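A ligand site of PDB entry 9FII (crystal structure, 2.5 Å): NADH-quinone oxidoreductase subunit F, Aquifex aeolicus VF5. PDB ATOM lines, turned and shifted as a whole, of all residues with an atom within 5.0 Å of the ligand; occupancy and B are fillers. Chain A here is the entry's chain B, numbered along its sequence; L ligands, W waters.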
ATOM      1  N   GLY A  65      18.220 -21.400  -2.490  1.00  0.00           N
ATOM      2  CA  GLY A  65      19.283 -21.409  -3.488  1.00  0.00           C
ATOM      3  C   GLY A  65      19.185 -22.628  -4.408  1.00  0.00           C
ATOM      4  O   GLY A  65      18.730 -23.688  -3.973  1.00  0.00           O
ATOM      5  N   ARG A  66      19.627 -22.472  -5.657  1.00  0.00           N
ATOM      6  CA  ARG A  66      19.507 -23.504  -6.680  1.00  0.00           C
ATOM      7  C   ARG A  66      20.853 -24.146  -6.986  1.00  0.00           C
ATOM      8  O   ARG A  66      20.932 -25.046  -7.820  1.00  0.00           O
ATOM      9  CB  ARG A  66      18.889 -22.891  -7.941  1.00  0.00           C
ATOM     10  CG  ARG A  66      17.497 -22.318  -7.734  1.00  0.00           C
ATOM     11  CD  ARG A  66      16.489 -23.347  -7.221  1.00  0.00           C
ATOM     12  NE  ARG A  66      15.119 -22.907  -7.502  1.00  0.00           N
ATOM     13  CZ  ARG A  66      14.175 -22.684  -6.604  1.00  0.00           C
ATOM     14  NH1 ARG A  66      12.948 -22.356  -6.991  1.00  0.00           N
ATOM     15  NH2 ARG A  66      14.436 -22.807  -5.319  1.00  0.00           N
ATOM     16  N   GLY A  67      21.909 -23.701  -6.294  1.00  0.00           N
ATOM     17  CA  GLY A  67      23.251 -24.211  -6.495  1.00  0.00           C
ATOM     18  C   GLY A  67      23.519 -25.506  -5.722  1.00  0.00           C
ATOM     19  O   GLY A  67      24.542 -26.124  -5.952  1.00  0.00           O
ATOM     20  N   GLY A  68      22.615 -25.908  -4.820  1.00  0.00           N
ATOM     21  CA  GLY A  68      22.736 -27.203  -4.179  1.00  0.00           C
ATOM     22  C   GLY A  68      22.314 -27.185  -2.712  1.00  0.00           C
ATOM     23  O   GLY A  68      21.494 -28.005  -2.311  1.00  0.00           O
ATOM     24  N   ALA A  69      22.898 -26.269  -1.933  1.00  0.00           N
ATOM     25  CA  ALA A  69      22.669 -26.231  -0.489  1.00  0.00           C
ATOM     26  C   ALA A  69      21.200 -25.977  -0.167  1.00  0.00           C
ATOM     27  O   ALA A  69      20.695 -26.504   0.822  1.00  0.00           O
ATOM     28  CB  ALA A  69      23.558 -25.179   0.144  1.00  0.00           C
ATOM     29  N   PHE A  71      19.984 -23.024   0.624  1.00  0.00           N
ATOM     30  CA  PHE A  71      19.934 -22.038   1.694  1.00  0.00           C
ATOM     31  C   PHE A  71      18.959 -20.929   1.310  1.00  0.00           C
ATOM     32  O   PHE A  71      18.994 -20.402   0.193  1.00  0.00           O
ATOM     33  CB  PHE A  71      21.336 -21.499   2.048  1.00  0.00           C
ATOM     34  CG  PHE A  71      21.374 -20.721   3.361  1.00  0.00           C
ATOM     35  CD1 PHE A  71      21.626 -21.364   4.567  1.00  0.00           C
ATOM     36  CD2 PHE A  71      21.090 -19.347   3.383  1.00  0.00           C
ATOM     37  CE1 PHE A  71      21.614 -20.643   5.756  1.00  0.00           C
ATOM     38  CE2 PHE A  71      21.078 -18.640   4.580  1.00  0.00           C
ATOM     39  CZ  PHE A  71      21.347 -19.286   5.759  1.00  0.00           C
ATOM     40  N   LYS A  76      20.149 -15.153   3.638  1.00  0.00           N
ATOM     41  CA  LYS A  76      21.517 -14.902   3.236  1.00  0.00           C
ATOM     42  C   LYS A  76      21.734 -13.400   3.002  1.00  0.00           C
ATOM     43  O   LYS A  76      22.769 -12.845   3.395  1.00  0.00           O
ATOM     44  CB  LYS A  76      21.856 -15.760   2.017  1.00  0.00           C
ATOM     45  CG  LYS A  76      23.286 -15.634   1.545  1.00  0.00           C
ATOM     46  CD  LYS A  76      23.546 -16.142   0.136  1.00  0.00           C
ATOM     47  CE  LYS A  76      23.460 -17.628   0.044  1.00  0.00           C
ATOM     48  NZ  LYS A  76      24.004 -18.024  -1.260  1.00  0.00           N
ATOM     49  N   ASN A  92      27.226 -16.967  -9.571  1.00  0.00           N
ATOM     50  CA  ASN A  92      27.966 -18.211  -9.739  1.00  0.00           C
ATOM     51  C   ASN A  92      27.529 -18.888 -11.038  1.00  0.00           C
ATOM     52  O   ASN A  92      26.428 -19.415 -11.131  1.00  0.00           O
ATOM     53  CB  ASN A  92      27.765 -19.119  -8.533  1.00  0.00           C
ATOM     54  CG  ASN A  92      28.816 -20.202  -8.424  1.00  0.00           C
ATOM     55  OD1 ASN A  92      29.509 -20.504  -9.391  1.00  0.00           O
ATOM     56  ND2 ASN A  92      28.954 -20.792  -7.240  1.00  0.00           N
ATOM     57  N   ASP A  94      29.745 -21.289 -12.686  1.00  0.00           N
ATOM     58  CA  ASP A  94      30.871 -22.190 -12.949  1.00  0.00           C
ATOM     59  C   ASP A  94      30.380 -23.512 -13.543  1.00  0.00           C
ATOM     60  O   ASP A  94      31.123 -24.127 -14.290  1.00  0.00           O
ATOM     61  CB  ASP A  94      31.765 -22.392 -11.744  1.00  0.00           C
ATOM     62  CG  ASP A  94      33.143 -22.957 -12.080  1.00  0.00           C
ATOM     63  OD1 ASP A  94      33.894 -22.280 -12.820  1.00  0.00           O
ATOM     64  OD2 ASP A  94      33.444 -24.092 -11.614  1.00  0.00           O
ATOM     65  N   GLU A  95      29.144 -23.915 -13.201  1.00  0.00           N
ATOM     66  CA  GLU A  95      28.502 -25.121 -13.695  1.00  0.00           C
ATOM     67  C   GLU A  95      29.485 -26.088 -14.360  1.00  0.00           C
ATOM     68  O   GLU A  95      29.635 -26.078 -15.588  1.00  0.00           O
ATOM     69  CB  GLU A  95      27.384 -24.751 -14.670  1.00  0.00           C
ATOM     70  CG  GLU A  95      26.528 -25.951 -15.070  1.00  0.00           C
ATOM     71  CD  GLU A  95      25.291 -25.627 -15.877  1.00  0.00           C
ATOM     72  OE1 GLU A  95      25.424 -25.085 -17.015  1.00  0.00           O
ATOM     73  OE2 GLU A  95      24.196 -25.925 -15.335  1.00  0.00           O
ATOM     74  N   SER A  96      30.119 -26.928 -13.530  1.00  0.00           N
ATOM     75  CA  SER A  96      31.120 -27.877 -13.975  1.00  0.00           C
ATOM     76  C   SER A  96      30.817 -29.291 -13.465  1.00  0.00           C
ATOM     77  O   SER A  96      31.587 -30.208 -13.769  1.00  0.00           O
ATOM     78  CB  SER A  96      32.493 -27.450 -13.561  1.00  0.00           C
ATOM     79  OG  SER A  96      32.881 -26.202 -14.109  1.00  0.00           O
ATOM     80  N   TYR A 180      36.722 -27.356 -11.308  1.00  0.00           N
ATOM     81  CA  TYR A 180      35.390 -27.579 -10.762  1.00  0.00           C
ATOM     82  C   TYR A 180      35.253 -26.920  -9.390  1.00  0.00           C
ATOM     83  O   TYR A 180      34.157 -26.506  -9.006  1.00  0.00           O
ATOM     84  CB  TYR A 180      35.166 -29.090 -10.722  1.00  0.00           C
ATOM     85  CG  TYR A 180      33.961 -29.516  -9.912  1.00  0.00           C
ATOM     86  CD1 TYR A 180      32.675 -29.112 -10.270  1.00  0.00           C
ATOM     87  CD2 TYR A 180      34.099 -30.330  -8.799  1.00  0.00           C
ATOM     88  CE1 TYR A 180      31.570 -29.488  -9.534  1.00  0.00           C
ATOM     89  CE2 TYR A 180      33.001 -30.734  -8.055  1.00  0.00           C
ATOM     90  CZ  TYR A 180      31.738 -30.297  -8.422  1.00  0.00           C
ATOM     91  OH  TYR A 180      30.639 -30.673  -7.736  1.00  0.00           O
ATOM     92  N   ILE A 181      36.367 -26.860  -8.640  1.00  0.00           N
ATOM     93  CA  ILE A 181      36.320 -26.401  -7.258  1.00  0.00           C
ATOM     94  C   ILE A 181      36.008 -24.906  -7.221  1.00  0.00           C
ATOM     95  O   ILE A 181      35.530 -24.419  -6.206  1.00  0.00           O
ATOM     96  CB  ILE A 181      37.616 -26.746  -6.477  1.00  0.00           C
ATOM     97  CG1 ILE A 181      37.407 -26.622  -4.961  1.00  0.00           C
ATOM     98  CG2 ILE A 181      38.809 -25.915  -6.928  1.00  0.00           C
ATOM     99  CD1 ILE A 181      36.381 -27.600  -4.381  1.00  0.00           C
ATOM    100  N   GLY A 183      33.649 -23.542  -8.301  1.00  0.00           N
ATOM    101  CA  GLY A 183      32.220 -23.396  -8.100  1.00  0.00           C
ATOM    102  C   GLY A 183      31.855 -23.326  -6.623  1.00  0.00           C
ATOM    103  O   GLY A 183      30.793 -22.813  -6.273  1.00  0.00           O
ATOM    104  N   GLU A 184      32.742 -23.855  -5.768  1.00  0.00           N
ATOM    105  CA  GLU A 184      32.606 -23.663  -4.331  1.00  0.00           C
ATOM    106  C   GLU A 184      32.823 -22.166  -4.076  1.00  0.00           C
ATOM    107  O   GLU A 184      33.758 -21.591  -4.620  1.00  0.00           O
ATOM    108  CB  GLU A 184      33.547 -24.612  -3.579  1.00  0.00           C
ATOM    109  CG  GLU A 184      33.225 -24.780  -2.089  1.00  0.00           C
ATOM    110  CD  GLU A 184      33.765 -23.660  -1.227  1.00  0.00           C
ATOM    111  OE1 GLU A 184      34.666 -22.966  -1.748  1.00  0.00           O
ATOM    112  OE2 GLU A 184      33.306 -23.438  -0.084  1.00  0.00           O
ATOM    113  N   GLU A 185      31.918 -21.540  -3.311  1.00  0.00           N
ATOM    114  CA  GLU A 185      31.763 -20.092  -3.332  1.00  0.00           C
ATOM    115  C   GLU A 185      33.045 -19.388  -2.851  1.00  0.00           C
ATOM    116  O   GLU A 185      33.425 -18.340  -3.376  1.00  0.00           O
ATOM    117  CB  GLU A 185      30.516 -19.608  -2.585  1.00  0.00           C
ATOM    118  CG  GLU A 185      30.435 -20.048  -1.133  1.00  0.00           C
ATOM    119  CD  GLU A 185      29.276 -19.449  -0.356  1.00  0.00           C
ATOM    120  OE1 GLU A 185      29.248 -19.819   0.830  1.00  0.00           O
ATOM    121  OE2 GLU A 185      28.446 -18.640  -0.851  1.00  0.00           O
ATOM    122  N   VAL A 218      27.185 -14.570  -2.765  1.00  0.00           N
ATOM    123  CA  VAL A 218      27.324 -15.425  -3.933  1.00  0.00           C
ATOM    124  C   VAL A 218      26.009 -16.164  -4.134  1.00  0.00           C
ATOM    125  O   VAL A 218      25.524 -16.844  -3.232  1.00  0.00           O
ATOM    126  CB  VAL A 218      28.486 -16.429  -3.775  1.00  0.00           C
ATOM    127  CG1 VAL A 218      28.706 -17.229  -5.045  1.00  0.00           C
ATOM    128  CG2 VAL A 218      29.791 -15.758  -3.352  1.00  0.00           C
ATOM    129  N   ASN A 219      25.408 -15.995  -5.337  1.00  0.00           N
ATOM    130  CA  ASN A 219      24.190 -16.713  -5.692  1.00  0.00           C
ATOM    131  C   ASN A 219      24.328 -17.348  -7.069  1.00  0.00           C
ATOM    132  O   ASN A 219      24.968 -16.790  -7.963  1.00  0.00           O
ATOM    133  CB  ASN A 219      22.966 -15.797  -5.663  1.00  0.00           C
ATOM    134  CG  ASN A 219      22.258 -15.799  -4.328  1.00  0.00           C
ATOM    135  OD1 ASN A 219      21.918 -14.731  -3.798  1.00  0.00           O
ATOM    136  ND2 ASN A 219      21.983 -16.985  -3.788  1.00  0.00           N
ATOM    137  N   ASN A 220      23.700 -18.516  -7.221  1.00  0.00           N
ATOM    138  CA  ASN A 220      23.642 -19.237  -8.479  1.00  0.00           C
ATOM    139  C   ASN A 220      22.752 -18.517  -9.502  1.00  0.00           C
ATOM    140  O   ASN A 220      21.777 -17.882  -9.136  1.00  0.00           O
ATOM    141  CB  ASN A 220      23.130 -20.667  -8.236  1.00  0.00           C
ATOM    142  CG  ASN A 220      22.969 -21.469  -9.497  1.00  0.00           C
ATOM    143  OD1 ASN A 220      21.835 -21.811  -9.876  1.00  0.00           O
ATOM    144  ND2 ASN A 220      24.072 -21.789 -10.178  1.00  0.00           N
ATOM    145  N   THR A 223      19.017 -19.028  -9.073  1.00  0.00           N
ATOM    146  CA  THR A 223      18.439 -18.367  -7.912  1.00  0.00           C
ATOM    147  C   THR A 223      18.105 -16.920  -8.292  1.00  0.00           C
ATOM    148  O   THR A 223      17.056 -16.405  -7.904  1.00  0.00           O
ATOM    149  CB  THR A 223      19.405 -18.395  -6.726  1.00  0.00           C
ATOM    150  OG1 THR A 223      19.773 -19.752  -6.528  1.00  0.00           O
ATOM    151  CG2 THR A 223      18.754 -17.818  -5.478  1.00  0.00           C
ATOM    152  N   CYS A 393      35.833 -28.508   2.897  1.00  0.00           N
ATOM    153  CA  CYS A 393      34.870 -28.202   1.855  1.00  0.00           C
ATOM    154  C   CYS A 393      34.164 -29.490   1.416  1.00  0.00           C
ATOM    155  O   CYS A 393      34.542 -30.594   1.809  1.00  0.00           O
ATOM    156  CB  CYS A 393      35.508 -27.493   0.662  1.00  0.00           C
ATOM    157  SG  CYS A 393      35.794 -28.534  -0.791  1.00  0.00           S
ATOM    158  N   GLY A 394      33.143 -29.339   0.583  1.00  0.00           N
ATOM    159  CA  GLY A 394      32.170 -30.393   0.373  1.00  0.00           C
ATOM    160  C   GLY A 394      32.647 -31.473  -0.592  1.00  0.00           C
ATOM    161  O   GLY A 394      32.070 -32.552  -0.595  1.00  0.00           O
ATOM    162  N   LEU A 395      33.675 -31.196  -1.421  1.00  0.00           N
ATOM    163  CA  LEU A 395      34.134 -32.132  -2.448  1.00  0.00           C
ATOM    164  C   LEU A 395      34.749 -33.371  -1.787  1.00  0.00           C
ATOM    165  O   LEU A 395      34.518 -34.503  -2.243  1.00  0.00           O
ATOM    166  CB  LEU A 395      35.131 -31.461  -3.389  1.00  0.00           C
ATOM    167  CG  LEU A 395      35.662 -32.316  -4.544  1.00  0.00           C
ATOM    168  CD1 LEU A 395      36.156 -31.487  -5.723  1.00  0.00           C
ATOM    169  CD2 LEU A 395      36.786 -33.212  -4.050  1.00  0.00           C
HETATM  170  N1  LIG L   1      27.202 -23.537  -6.737  1.00  0.00           N
HETATM  171  C1  LIG L   1      26.854 -23.035  -7.960  1.00  0.00           C
HETATM  172  O1  LIG L   1      25.976 -22.175  -8.067  1.00  0.00           O
HETATM  173  N2  LIG L   1      27.514 -23.498  -9.097  1.00  0.00           N
HETATM  174  C2  LIG L   1      28.500 -24.466  -9.137  1.00  0.00           C
HETATM  175  O2  LIG L   1      28.995 -24.830 -10.205  1.00  0.00           O
HETATM  176  C3  LIG L   1      28.879 -24.980  -7.852  1.00  0.00           C
HETATM  177  N3  LIG L   1      29.851 -25.837  -7.788  1.00  0.00           N
HETATM  178  C4  LIG L   1      30.239 -26.279  -6.541  1.00  0.00           C
HETATM  179  C5  LIG L   1      31.326 -27.151  -6.467  1.00  0.00           C
HETATM  180  C6  LIG L   1      31.778 -27.627  -5.244  1.00  0.00           C
HETATM  181  C7  LIG L   1      32.978 -28.535  -5.211  1.00  0.00           C
HETATM  182  C8  LIG L   1      31.125 -27.244  -4.060  1.00  0.00           C
HETATM  183  C9  LIG L   1      31.528 -27.815  -2.735  1.00  0.00           C
HETATM  184  C10 LIG L   1      30.053 -26.365  -4.132  1.00  0.00           C
HETATM  185  C11 LIG L   1      29.605 -25.856  -5.355  1.00  0.00           C
HETATM  186  N4  LIG L   1      28.550 -24.914  -5.446  1.00  0.00           N
HETATM  187  C12 LIG L   1      28.166 -24.454  -6.685  1.00  0.00           C
HETATM  188  C13 LIG L   1      27.883 -24.366  -4.274  1.00  0.00           C
HETATM  189  C14 LIG L   1      28.381 -22.964  -3.927  1.00  0.00           C
HETATM  190  O3  LIG L   1      29.535 -23.020  -3.088  1.00  0.00           O
HETATM  191  C15 LIG L   1      27.304 -22.112  -3.242  1.00  0.00           C
HETATM  192  O4  LIG L   1      26.596 -22.870  -2.254  1.00  0.00           O
HETATM  193  C16 LIG L   1      26.272 -21.502  -4.190  1.00  0.00           C
HETATM  194  O5  LIG L   1      26.934 -20.877  -5.284  1.00  0.00           O
HETATM  195  C17 LIG L   1      25.423 -20.498  -3.444  1.00  0.00           C
HETATM  196  O6  LIG L   1      24.446 -19.911  -4.314  1.00  0.00           O
HETATM  197  P1  LIG L   1      22.885 -20.297  -4.073  1.00  0.00           P
HETATM  198  O7  LIG L   1      22.680 -21.801  -4.174  1.00  0.00           O
HETATM  199  O8  LIG L   1      22.466 -19.777  -2.748  1.00  0.00           O
HETATM  200  O9  LIG L   1      22.184 -19.536  -5.234  1.00  0.00           O
HETATM  201  O   HOH W   1      26.807 -22.112 -11.736  1.00  0.00           O
HETATM  202  O   HOH W   2      25.806 -26.484  -8.742  1.00  0.00           O
HETATM  203  O   HOH W   3      31.414 -25.902 -10.322  1.00  0.00           O
HETATM  204  O   HOH W   4      20.238 -18.730  -1.621  1.00  0.00           O
HETATM  205  O   HOH W   5      27.249 -27.527 -11.313  1.00  0.00           O
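The backbone carbonyl oxygen (O) of Val 218 lies close to an oxygen (O6) of the ligand. Gly 65 touches the ligand. C of Asp 94 touches O2 of the ligand (3.8 Å). CE2 of Tyr 180 touches C7 of the ligand (3.6 Å). Ile 181 touches the ligand (CD1 to C7, 3.6 Å). Glu 184 touches the ligand (CA to O3, 3.4 Å). Gly 394 touches the ligand (N to C9, 3.99 Å). Hydrophobic or aromatic side chains that line the ligand: Tyr 180 and Ile 181. 17 residues have an atom within 4 Å of the ligand: Gly 65, Arg 66, Gly 67, Lys 76, Asn 92, Asp 94, Glu 95, Tyr 180, Ile 181, Gly 183, Glu 184, Glu 185, Val 218, Asn 219, Asn 220, Thr 223 and Gly 394. The nearest printed residue that does not touch the ligand is Leu 395 (4.1 Å).
N of Asn 92 is in hydrogen-bond range of O of Asn 219 (2.8 Å). ND2 of Asn 220 lies within hydrogen-bond range of O of Asn 92. The side-chain amino group of Lys 76 sits close to the side-chain amide nitrogen of Asn 219. OD2 of Asp 94 is in hydrogen-bond range of N of Gly 183. N of Asp 94 lies within hydrogen-bond range of OD1 of Asn 92, 3.4 Å away. NZ of Lys 76 is in hydrogen-bond range of O of Val 218. The backbone carbonyl oxygen (O) of Asp 94 lies within hydrogen-bond range of the side-chain hydroxyl (OG) of Ser 96 (2.7 Å). ND2 of Asn 92 is in hydrogen-bond range of O of Gly 183 (2.9 Å).
An oxygen (O9) of the ligand lies within hydrogen-bond range of the side-chain amide nitrogen of Asn 219 (2.9 Å). N of Glu 185 sits at hydrogen-bond distance from O3 of the ligand, 2.8 Å away. The backbone NH of Gly 67 is in hydrogen-bond range of an oxygen (O7) of the ligand, at 2.9 Å. ND2 of Asn 92 lies within hydrogen-bond range of O5 of the ligand (2.8 Å). OG1 of Thr 223 lies within hydrogen-bond range of O9 of the ligand (2.7 Å). N of Arg 66 is in hydrogen-bond range of O7 of the ligand (3.5 Å). O9 of the ligand sits at hydrogen-bond distance from N of Asn 220 (2.7 Å). O2 of the ligand sits at hydrogen-bond distance from N of Glu 95, 3.1 Å away. An oxygen (O8) of the ligand lies within salt-bridge range of the side-chain amino group (NZ) of Lys 76 (2.8 Å). The side-chain amide nitrogen (ND2) of Asn 220 is in hydrogen-bond range of an oxygen (O1) of the ligand, at 2.9 Å. O3 of the ligand lies close to O of Gly 183, 3.4 Å away.
Water W4 lies within hydrogen-bond range of an oxygen (O8) of the ligand, the backbone carbonyl oxygen of Phe 71, the side-chain amide nitrogen of Asn 219 and the backbone NH of Gly 65. Water W2 bridges the backbone carbonyl oxygen of Gly 67 and a nitrogen (N2) of the ligand.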
